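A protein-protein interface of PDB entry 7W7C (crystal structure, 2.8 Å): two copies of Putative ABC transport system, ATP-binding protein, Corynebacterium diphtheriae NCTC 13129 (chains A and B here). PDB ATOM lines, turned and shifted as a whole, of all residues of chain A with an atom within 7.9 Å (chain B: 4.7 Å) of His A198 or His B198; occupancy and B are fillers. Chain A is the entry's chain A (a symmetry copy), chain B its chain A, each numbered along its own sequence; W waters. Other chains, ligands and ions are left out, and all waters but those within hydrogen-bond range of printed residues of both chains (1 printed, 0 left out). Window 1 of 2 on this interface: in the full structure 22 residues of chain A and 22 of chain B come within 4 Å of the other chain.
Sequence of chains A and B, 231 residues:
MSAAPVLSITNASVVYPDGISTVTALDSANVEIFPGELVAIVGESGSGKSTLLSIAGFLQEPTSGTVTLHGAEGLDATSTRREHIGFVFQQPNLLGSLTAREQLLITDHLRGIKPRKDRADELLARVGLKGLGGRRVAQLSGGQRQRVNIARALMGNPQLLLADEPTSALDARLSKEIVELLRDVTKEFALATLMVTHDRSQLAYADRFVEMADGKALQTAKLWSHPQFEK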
ATOM      1  N   ILE A  41     -26.130  35.193  -7.899  1.00  0.00           N
ATOM      2  CA  ILE A  41     -25.052  34.464  -8.560  1.00  0.00           C
ATOM      3  C   ILE A  41     -25.253  32.985  -8.260  1.00  0.00           C
ATOM      4  O   ILE A  41     -25.248  32.579  -7.092  1.00  0.00           O
ATOM      5  CB  ILE A  41     -23.676  34.934  -8.068  1.00  0.00           C
ATOM      6  CG1 ILE A  41     -23.627  36.461  -7.983  1.00  0.00           C
ATOM      7  CG2 ILE A  41     -22.578  34.417  -8.981  1.00  0.00           C
ATOM      8  CD1 ILE A  41     -22.495  36.982  -7.120  1.00  0.00           C
ATOM      9  N   VAL A  42     -25.443  32.177  -9.302  1.00  0.00           N
ATOM     10  CA  VAL A  42     -25.725  30.760  -9.125  1.00  0.00           C
ATOM     11  C   VAL A  42     -24.721  29.940  -9.918  1.00  0.00           C
ATOM     12  O   VAL A  42     -24.036  30.444 -10.805  1.00  0.00           O
ATOM     13  CB  VAL A  42     -27.162  30.396  -9.539  1.00  0.00           C
ATOM     14  CG1 VAL A  42     -28.123  30.919  -8.502  1.00  0.00           C
ATOM     15  CG2 VAL A  42     -27.478  30.970 -10.905  1.00  0.00           C
ATOM     16  N   GLY A  43     -24.625  28.663  -9.562  1.00  0.00           N
ATOM     17  CA  GLY A  43     -23.684  27.754 -10.189  1.00  0.00           C
ATOM     18  C   GLY A  43     -23.114  26.732  -9.230  1.00  0.00           C
ATOM     19  O   GLY A  43     -22.950  27.010  -8.039  1.00  0.00           O
ATOM     20  N   GLU A  44     -22.806  25.542  -9.751  1.00  0.00           N
ATOM     21  CA  GLU A  44     -22.227  24.452  -8.974  1.00  0.00           C
ATOM     22  C   GLU A  44     -20.998  24.898  -8.191  1.00  0.00           C
ATOM     23  O   GLU A  44     -20.328  25.865  -8.573  1.00  0.00           O
ATOM     24  CB  GLU A  44     -21.870  23.279  -9.897  1.00  0.00           C
ATOM     25  CG  GLU A  44     -23.088  22.508 -10.400  1.00  0.00           C
ATOM     26  CD  GLU A  44     -22.756  21.426 -11.402  1.00  0.00           C
ATOM     27  OE1 GLU A  44     -21.612  21.397 -11.909  1.00  0.00           O
ATOM     28  OE2 GLU A  44     -23.657  20.602 -11.681  1.00  0.00           O
ATOM     29  N   SER A  45     -20.699  24.203  -7.098  1.00  0.00           N
ATOM     30  CA  SER A  45     -19.567  24.570  -6.256  1.00  0.00           C
ATOM     31  C   SER A  45     -18.274  24.538  -7.060  1.00  0.00           C
ATOM     32  O   SER A  45     -18.076  23.673  -7.914  1.00  0.00           O
ATOM     33  CB  SER A  45     -19.465  23.616  -5.064  1.00  0.00           C
ATOM     34  OG  SER A  45     -19.101  22.317  -5.497  1.00  0.00           O
ATOM     35  N   GLY A  46     -17.394  25.496  -6.792  1.00  0.00           N
ATOM     36  CA  GLY A  46     -16.139  25.568  -7.514  1.00  0.00           C
ATOM     37  C   GLY A  46     -16.202  26.236  -8.870  1.00  0.00           C
ATOM     38  O   GLY A  46     -15.301  26.027  -9.687  1.00  0.00           O
ATOM     39  N   SER A  47     -17.232  27.039  -9.138  1.00  0.00           N
ATOM     40  CA  SER A  47     -17.342  27.753 -10.403  1.00  0.00           C
ATOM     41  C   SER A  47     -17.081  29.246 -10.259  1.00  0.00           C
ATOM     42  O   SER A  47     -17.330  30.003 -11.205  1.00  0.00           O
ATOM     43  CB  SER A  47     -18.712  27.509 -11.038  1.00  0.00           C
ATOM     44  OG  SER A  47     -19.753  27.996 -10.209  1.00  0.00           O
ATOM     45  N   LYS A  49     -18.213  31.523  -7.730  1.00  0.00           N
ATOM     46  CA  LYS A  49     -19.225  32.411  -7.170  1.00  0.00           C
ATOM     47  C   LYS A  49     -18.625  33.312  -6.093  1.00  0.00           C
ATOM     48  O   LYS A  49     -18.685  34.546  -6.185  1.00  0.00           O
ATOM     49  CB  LYS A  49     -20.387  31.592  -6.611  1.00  0.00           C
ATOM     50  CG  LYS A  49     -21.135  30.767  -7.643  1.00  0.00           C
ATOM     51  CD  LYS A  49     -22.432  30.228  -7.058  1.00  0.00           C
ATOM     52  CE  LYS A  49     -22.186  29.381  -5.816  1.00  0.00           C
ATOM     53  NZ  LYS A  49     -21.774  27.985  -6.104  1.00  0.00           N
ATOM     54  N   GLU A 165     -24.198  33.246   0.562  1.00  0.00           N
ATOM     55  CA  GLU A 165     -24.978  32.092   1.005  1.00  0.00           C
ATOM     56  C   GLU A 165     -25.385  32.203   2.483  1.00  0.00           C
ATOM     57  O   GLU A 165     -25.044  31.328   3.285  1.00  0.00           O
ATOM     58  CB  GLU A 165     -24.215  30.795   0.749  1.00  0.00           C
ATOM     59  CG  GLU A 165     -24.543  30.097  -0.570  1.00  0.00           C
ATOM     60  CD  GLU A 165     -25.746  29.172  -0.461  1.00  0.00           C
ATOM     61  OE1 GLU A 165     -26.624  29.437   0.383  1.00  0.00           O
ATOM     62  OE2 GLU A 165     -25.817  28.175  -1.208  1.00  0.00           O
ATOM     63  N   THR A 167     -27.934  31.621   4.183  1.00  0.00           N
ATOM     64  CA  THR A 167     -28.872  30.647   4.725  1.00  0.00           C
ATOM     65  C   THR A 167     -28.295  29.237   4.732  1.00  0.00           C
ATOM     66  O   THR A 167     -29.050  28.274   4.907  1.00  0.00           O
ATOM     67  CB  THR A 167     -30.186  30.663   3.936  1.00  0.00           C
ATOM     68  OG1 THR A 167     -30.006  29.973   2.690  1.00  0.00           O
ATOM     69  CG2 THR A 167     -30.624  32.091   3.663  1.00  0.00           C
ATOM     70  N   MET A 195     -26.230  38.385  -4.331  1.00  0.00           N
ATOM     71  CA  MET A 195     -26.450  37.268  -3.419  1.00  0.00           C
ATOM     72  C   MET A 195     -25.995  35.974  -4.073  1.00  0.00           C
ATOM     73  O   MET A 195     -26.507  35.601  -5.130  1.00  0.00           O
ATOM     74  CB  MET A 195     -27.916  37.157  -3.014  1.00  0.00           C
ATOM     75  CG  MET A 195     -28.183  36.052  -1.991  1.00  0.00           C
ATOM     76  SD  MET A 195     -29.936  35.842  -1.642  1.00  0.00           S
ATOM     77  CE  MET A 195     -30.506  35.296  -3.245  1.00  0.00           C
ATOM     78  N   VAL A 196     -25.055  35.287  -3.438  1.00  0.00           N
ATOM     79  CA  VAL A 196     -24.612  33.969  -3.879  1.00  0.00           C
ATOM     80  C   VAL A 196     -25.468  32.912  -3.196  1.00  0.00           C
ATOM     81  O   VAL A 196     -25.607  32.919  -1.968  1.00  0.00           O
ATOM     82  CB  VAL A 196     -23.125  33.754  -3.556  1.00  0.00           C
ATOM     83  CG1 VAL A 196     -22.704  32.352  -3.909  1.00  0.00           C
ATOM     84  CG2 VAL A 196     -22.271  34.776  -4.272  1.00  0.00           C
ATOM     85  N   THR A 197     -26.043  32.005  -3.981  1.00  0.00           N
ATOM     86  CA  THR A 197     -26.750  30.867  -3.417  1.00  0.00           C
ATOM     87  C   THR A 197     -26.599  29.654  -4.318  1.00  0.00           C
ATOM     88  O   THR A 197     -26.311  29.763  -5.514  1.00  0.00           O
ATOM     89  CB  THR A 197     -28.245  31.138  -3.194  1.00  0.00           C
ATOM     90  OG1 THR A 197     -28.891  29.926  -2.796  1.00  0.00           O
ATOM     91  CG2 THR A 197     -28.890  31.659  -4.469  1.00  0.00           C
ATOM     92  N   HIS A 198     -26.808  28.488  -3.710  1.00  0.00           N
ATOM     93  CA  HIS A 198     -26.851  27.220  -4.417  1.00  0.00           C
ATOM     94  C   HIS A 198     -28.220  26.560  -4.339  1.00  0.00           C
ATOM     95  O   HIS A 198     -28.435  25.528  -4.983  1.00  0.00           O
ATOM     96  CB  HIS A 198     -25.783  26.270  -3.866  1.00  0.00           C
ATOM     97  CG  HIS A 198     -25.401  25.181  -4.820  1.00  0.00           C
ATOM     98  ND1 HIS A 198     -26.074  24.959  -6.002  1.00  0.00           N
ATOM     99  CD2 HIS A 198     -24.411  24.259  -4.772  1.00  0.00           C
ATOM    100  CE1 HIS A 198     -25.521  23.942  -6.637  1.00  0.00           C
ATOM    101  NE2 HIS A 198     -24.510  23.499  -5.913  1.00  0.00           N
ATOM    102  N   ASP A 199     -29.156  27.141  -3.597  1.00  0.00           N
ATOM    103  CA  ASP A 199     -30.470  26.552  -3.380  1.00  0.00           C
ATOM    104  C   ASP A 199     -31.469  27.197  -4.332  1.00  0.00           C
ATOM    105  O   ASP A 199     -31.711  28.405  -4.261  1.00  0.00           O
ATOM    106  CB  ASP A 199     -30.908  26.732  -1.929  1.00  0.00           C
ATOM    107  CG  ASP A 199     -29.929  26.116  -0.951  1.00  0.00           C
ATOM    108  OD1 ASP A 199     -29.383  25.036  -1.270  1.00  0.00           O
ATOM    109  OD2 ASP A 199     -29.693  26.721   0.118  1.00  0.00           O
ATOM    110  N   ARG A 200     -32.055  26.384  -5.210  1.00  0.00           N
ATOM    111  CA  ARG A 200     -32.957  26.921  -6.221  1.00  0.00           C
ATOM    112  C   ARG A 200     -34.269  27.395  -5.610  1.00  0.00           C
ATOM    113  O   ARG A 200     -34.930  28.279  -6.171  1.00  0.00           O
ATOM    114  CB  ARG A 200     -33.187  25.879  -7.314  1.00  0.00           C
ATOM    115  CG  ARG A 200     -31.915  25.551  -8.100  1.00  0.00           C
ATOM    116  CD  ARG A 200     -31.124  26.828  -8.347  1.00  0.00           C
ATOM    117  NE  ARG A 200     -29.939  26.651  -9.183  1.00  0.00           N
ATOM    118  CZ  ARG A 200     -29.954  26.688 -10.512  1.00  0.00           C
ATOM    119  NH1 ARG A 200     -31.099  26.876 -11.153  1.00  0.00           N
ATOM    120  NH2 ARG A 200     -28.829  26.532 -11.198  1.00  0.00           N
ATOM    121  N   SER A 201     -34.636  26.864  -4.439  1.00  0.00           N
ATOM    122  CA  SER A 201     -35.802  27.325  -3.689  1.00  0.00           C
ATOM    123  C   SER A 201     -35.706  28.809  -3.355  1.00  0.00           C
ATOM    124  O   SER A 201     -36.634  29.383  -2.775  1.00  0.00           O
ATOM    125  CB  SER A 201     -35.962  26.523  -2.394  1.00  0.00           C
ATOM    126  OG  SER A 201     -34.917  26.807  -1.475  1.00  0.00           O
ATOM    127  N   GLN A 202     -34.581  29.435  -3.700  1.00  0.00           N
ATOM    128  CA  GLN A 202     -34.369  30.848  -3.446  1.00  0.00           C
ATOM    129  C   GLN A 202     -34.423  31.714  -4.697  1.00  0.00           C
ATOM    130  O   GLN A 202     -34.652  32.922  -4.576  1.00  0.00           O
ATOM    131  CB  GLN A 202     -33.017  31.059  -2.747  1.00  0.00           C
ATOM    132  CG  GLN A 202     -32.843  30.234  -1.476  1.00  0.00           C
ATOM    133  CD  GLN A 202     -31.879  30.874  -0.496  1.00  0.00           C
ATOM    134  OE1 GLN A 202     -32.038  30.756   0.720  1.00  0.00           O
ATOM    135  NE2 GLN A 202     -30.877  31.564  -1.022  1.00  0.00           N
ATOM    136  N   LEU A 203     -34.255  31.131  -5.889  1.00  0.00           N
ATOM    137  CA  LEU A 203     -34.110  31.948  -7.092  1.00  0.00           C
ATOM    138  C   LEU A 203     -35.349  32.785  -7.375  1.00  0.00           C
ATOM    139  O   LEU A 203     -35.258  33.826  -8.036  1.00  0.00           O
ATOM    140  CB  LEU A 203     -33.782  31.066  -8.296  1.00  0.00           C
ATOM    141  CG  LEU A 203     -32.329  30.595  -8.318  1.00  0.00           C
ATOM    142  CD1 LEU A 203     -31.955  30.037  -9.684  1.00  0.00           C
ATOM    143  CD2 LEU A 203     -31.410  31.744  -7.918  1.00  0.00           C
ATOM    144  N   GLY B  43     -29.378  17.333  -0.819  1.00  0.00           N
ATOM    145  CA  GLY B  43     -30.305  18.247  -0.178  1.00  0.00           C
ATOM    146  C   GLY B  43     -29.755  19.649  -0.035  1.00  0.00           C
ATOM    147  O   GLY B  43     -28.546  19.838   0.125  1.00  0.00           O
ATOM    148  N   GLU B  44     -30.648  20.641  -0.090  1.00  0.00           N
ATOM    149  CA  GLU B  44     -30.293  22.048   0.053  1.00  0.00           C
ATOM    150  C   GLU B  44     -29.458  22.304   1.301  1.00  0.00           C
ATOM    151  O   GLU B  44     -29.529  21.540   2.272  1.00  0.00           O
ATOM    152  CB  GLU B  44     -31.562  22.911   0.079  1.00  0.00           C
ATOM    153  CG  GLU B  44     -32.239  23.037  -1.284  1.00  0.00           C
ATOM    154  CD  GLU B  44     -33.552  23.786  -1.247  1.00  0.00           C
ATOM    155  OE1 GLU B  44     -34.087  24.023  -0.140  1.00  0.00           O
ATOM    156  OE2 GLU B  44     -34.048  24.136  -2.343  1.00  0.00           O
ATOM    157  N   SER B  45     -28.664  23.370   1.284  1.00  0.00           N
ATOM    158  CA  SER B  45     -27.794  23.684   2.411  1.00  0.00           C
ATOM    159  C   SER B  45     -28.616  23.876   3.679  1.00  0.00           C
ATOM    160  O   SER B  45     -29.714  24.436   3.649  1.00  0.00           O
ATOM    161  CB  SER B  45     -26.984  24.947   2.116  1.00  0.00           C
ATOM    162  OG  SER B  45     -27.831  26.082   2.074  1.00  0.00           O
ATOM    163  N   GLU B 165     -18.339  16.647   0.341  1.00  0.00           N
ATOM    164  CA  GLU B 165     -18.265  17.562  -0.797  1.00  0.00           C
ATOM    165  C   GLU B 165     -16.817  17.804  -1.250  1.00  0.00           C
ATOM    166  O   GLU B 165     -16.358  18.951  -1.266  1.00  0.00           O
ATOM    167  CB  GLU B 165     -18.961  18.881  -0.475  1.00  0.00           C
ATOM    168  CG  GLU B 165     -20.421  18.972  -0.916  1.00  0.00           C
ATOM    169  CD  GLU B 165     -20.572  19.436  -2.357  1.00  0.00           C
ATOM    170  OE1 GLU B 165     -19.653  19.186  -3.160  1.00  0.00           O
ATOM    171  OE2 GLU B 165     -21.599  20.060  -2.691  1.00  0.00           O
ATOM    172  N   VAL B 196     -21.416  13.270   0.470  1.00  0.00           N
ATOM    173  CA  VAL B 196     -22.280  14.444   0.496  1.00  0.00           C
ATOM    174  C   VAL B 196     -21.946  15.324  -0.700  1.00  0.00           C
ATOM    175  O   VAL B 196     -20.777  15.667  -0.916  1.00  0.00           O
ATOM    176  CB  VAL B 196     -22.105  15.224   1.808  1.00  0.00           C
ATOM    177  CG1 VAL B 196     -22.912  16.495   1.780  1.00  0.00           C
ATOM    178  CG2 VAL B 196     -22.483  14.364   2.994  1.00  0.00           C
ATOM    179  N   THR B 197     -22.960  15.691  -1.479  1.00  0.00           N
ATOM    180  CA  THR B 197     -22.769  16.653  -2.552  1.00  0.00           C
ATOM    181  C   THR B 197     -24.022  17.492  -2.735  1.00  0.00           C
ATOM    182  O   THR B 197     -25.127  17.104  -2.343  1.00  0.00           O
ATOM    183  CB  THR B 197     -22.411  15.996  -3.892  1.00  0.00           C
ATOM    184  OG1 THR B 197     -22.404  16.991  -4.920  1.00  0.00           O
ATOM    185  CG2 THR B 197     -23.418  14.913  -4.244  1.00  0.00           C
ATOM    186  N   HIS B 198     -23.820  18.655  -3.350  1.00  0.00           N
ATOM    187  CA  HIS B 198     -24.899  19.542  -3.747  1.00  0.00           C
ATOM    188  C   HIS B 198     -24.986  19.707  -5.258  1.00  0.00           C
ATOM    189  O   HIS B 198     -25.923  20.348  -5.746  1.00  0.00           O
ATOM    190  CB  HIS B 198     -24.732  20.912  -3.083  1.00  0.00           C
ATOM    191  CG  HIS B 198     -26.004  21.698  -3.004  1.00  0.00           C
ATOM    192  ND1 HIS B 198     -27.165  21.296  -3.628  1.00  0.00           N
ATOM    193  CD2 HIS B 198     -26.300  22.856  -2.369  1.00  0.00           C
ATOM    194  CE1 HIS B 198     -28.120  22.177  -3.387  1.00  0.00           C
ATOM    195  NE2 HIS B 198     -27.621  23.134  -2.626  1.00  0.00           N
ATOM    196  N   ASP B 199     -24.058  19.123  -6.008  1.00  0.00           N
ATOM    197  CA  ASP B 199     -23.993  19.287  -7.453  1.00  0.00           C
ATOM    198  C   ASP B 199     -24.641  18.083  -8.122  1.00  0.00           C
ATOM    199  O   ASP B 199     -24.170  16.952  -7.968  1.00  0.00           O
ATOM    200  CB  ASP B 199     -22.546  19.450  -7.912  1.00  0.00           C
ATOM    201  CG  ASP B 199     -21.862  20.632  -7.254  1.00  0.00           C
ATOM    202  OD1 ASP B 199     -22.538  21.668  -7.062  1.00  0.00           O
ATOM    203  OD2 ASP B 199     -20.665  20.514  -6.912  1.00  0.00           O
ATOM    204  N   ARG B 200     -25.712  18.333  -8.875  1.00  0.00           N
ATOM    205  CA  ARG B 200     -26.455  17.236  -9.483  1.00  0.00           C
ATOM    206  C   ARG B 200     -25.670  16.583 -10.613  1.00  0.00           C
ATOM    207  O   ARG B 200     -25.885  15.401 -10.913  1.00  0.00           O
ATOM    208  CB  ARG B 200     -27.818  17.737  -9.957  1.00  0.00           C
ATOM    209  CG  ARG B 200     -28.718  18.191  -8.806  1.00  0.00           C
ATOM    210  CD  ARG B 200     -28.567  17.234  -7.631  1.00  0.00           C
ATOM    211  NE  ARG B 200     -29.463  17.510  -6.510  1.00  0.00           N
ATOM    212  CZ  ARG B 200     -30.704  17.045  -6.418  1.00  0.00           C
ATOM    213  NH1 ARG B 200     -31.203  16.299  -7.394  1.00  0.00           N
ATOM    214  NH2 ARG B 200     -31.449  17.331  -5.357  1.00  0.00           N
HETATM  215  O   HOH W   1     -30.735  26.872   3.586  1.00  0.00           O
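The side-chain hydroxyl (OG) of Ser A201 sits at hydrogen-bond distance from the side-chain carboxylate (OE2) of Glu B44 (2.9 Å).
The side-chain carboxylate (OD1) of Asp B199 is in hydrogen-bond range of a ring nitrogen (NE2) of His A198 (2.9 Å).
The side-chain carboxylate of Asp B199 lies within hydrogen-bond range of the side-chain hydroxyl of Ser A45 (2.8 Å).
O of His B198 lies within hydrogen-bond range of NE2 of His A198 (3.5 Å).
OG of Ser B45 is in hydrogen-bond range of OD2 of Asp A199 (2.8 Å).
OD1 of Asp A199 lies within hydrogen-bond range of NE2 of His B198 (2.9 Å).
The backbone NH (N) of Asp A199 lies within hydrogen-bond range of the side-chain hydroxyl (OG1) of Thr A197, at 2.9 Å.
OG of Ser A47 lies within hydrogen-bond range of O of Glu A44.
The backbone NH (N) of His B198 is in hydrogen-bond range of the side-chain carboxylate (OE2) of Glu B165 (2.7 Å).
OE1 of Gln A202 lies within hydrogen-bond range of OG1 of Thr A167 (2.9 Å).
The backbone NH of Glu A165 is in hydrogen-bond range of the backbone carbonyl oxygen of Val A196 (2.9 Å).
OG1 of Thr B197 lies within hydrogen-bond range of N of Asp B199.
Among the printed residues, merely in contact across the chains: Glu A44 with Asp B199 (3.3 Å), Asp A199 with Glu B44 (3.3 Å), Thr A167 with Ser B45 (3.8 Å), Ser A45 with Glu B165 (3.9 Å) and Glu A165 with Ser B45 (3.9 Å).
Of the printed residues of chain B, Ser A45 touches Glu B165 (3.9 Å) and Asp B199 (2.8 Å).
Printed residues of chain B within 4 Å of Glu A165: Ser B45.
Val A196 touches none of the printed residues of chain B.
Printed residues of chain B within 4 Å of His A198: His B198 and Asp B199.
Of the printed residues of chain B, Asp A199 touches Glu B44 (3.3 Å), Ser B45 (2.8 Å) and His B198 (2.9 Å).
Of chain A, only His A198 and Asp A199 come within 4 Å of His B198.
Of the 19 printed residues of chain A, 7 touch a printed residue of chain B.
Of the 9 printed residues of chain B, 5 touch a printed residue of chain A.
Printed residues of chain B that touch a printed residue of chain A: Glu B44, Ser B45, Glu B165, His B198 and Asp B199.
Hydrophobic or aromatic side chains of chain B within 4 Å of the printed part of chain A: His B198.
Among the printed residues, no Asp or Glu carboxylate lies within 4 Å of a Lys or Arg side-chain nitrogen of the other chain.
Glu A44 touches Asp B199, and with the chains exchanged Asp A199 touches Glu B44.
Ser A45 touches Glu B165, and with the chains exchanged Glu A165 touches Ser B45.
Ser A45 touches Asp B199, and with the chains exchanged Asp A199 touches Ser B45.
His A198 touches Asp B199, and with the chains exchanged Asp A199 touches His B198.
Positions printed for both chains: 43, 44, 45, 165, 196, 197, 198, 199 and 200.
Of the 11 pairs that touch across the chains among the printed residues, 9 have their exchanged pair printed and touching as well.
Water W1 lies within hydrogen-bond range of the backbone carbonyl oxygen of Thr A167 (2.6 Å) and the backbone carbonyl oxygen of Ser B45 (2.6 Å).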
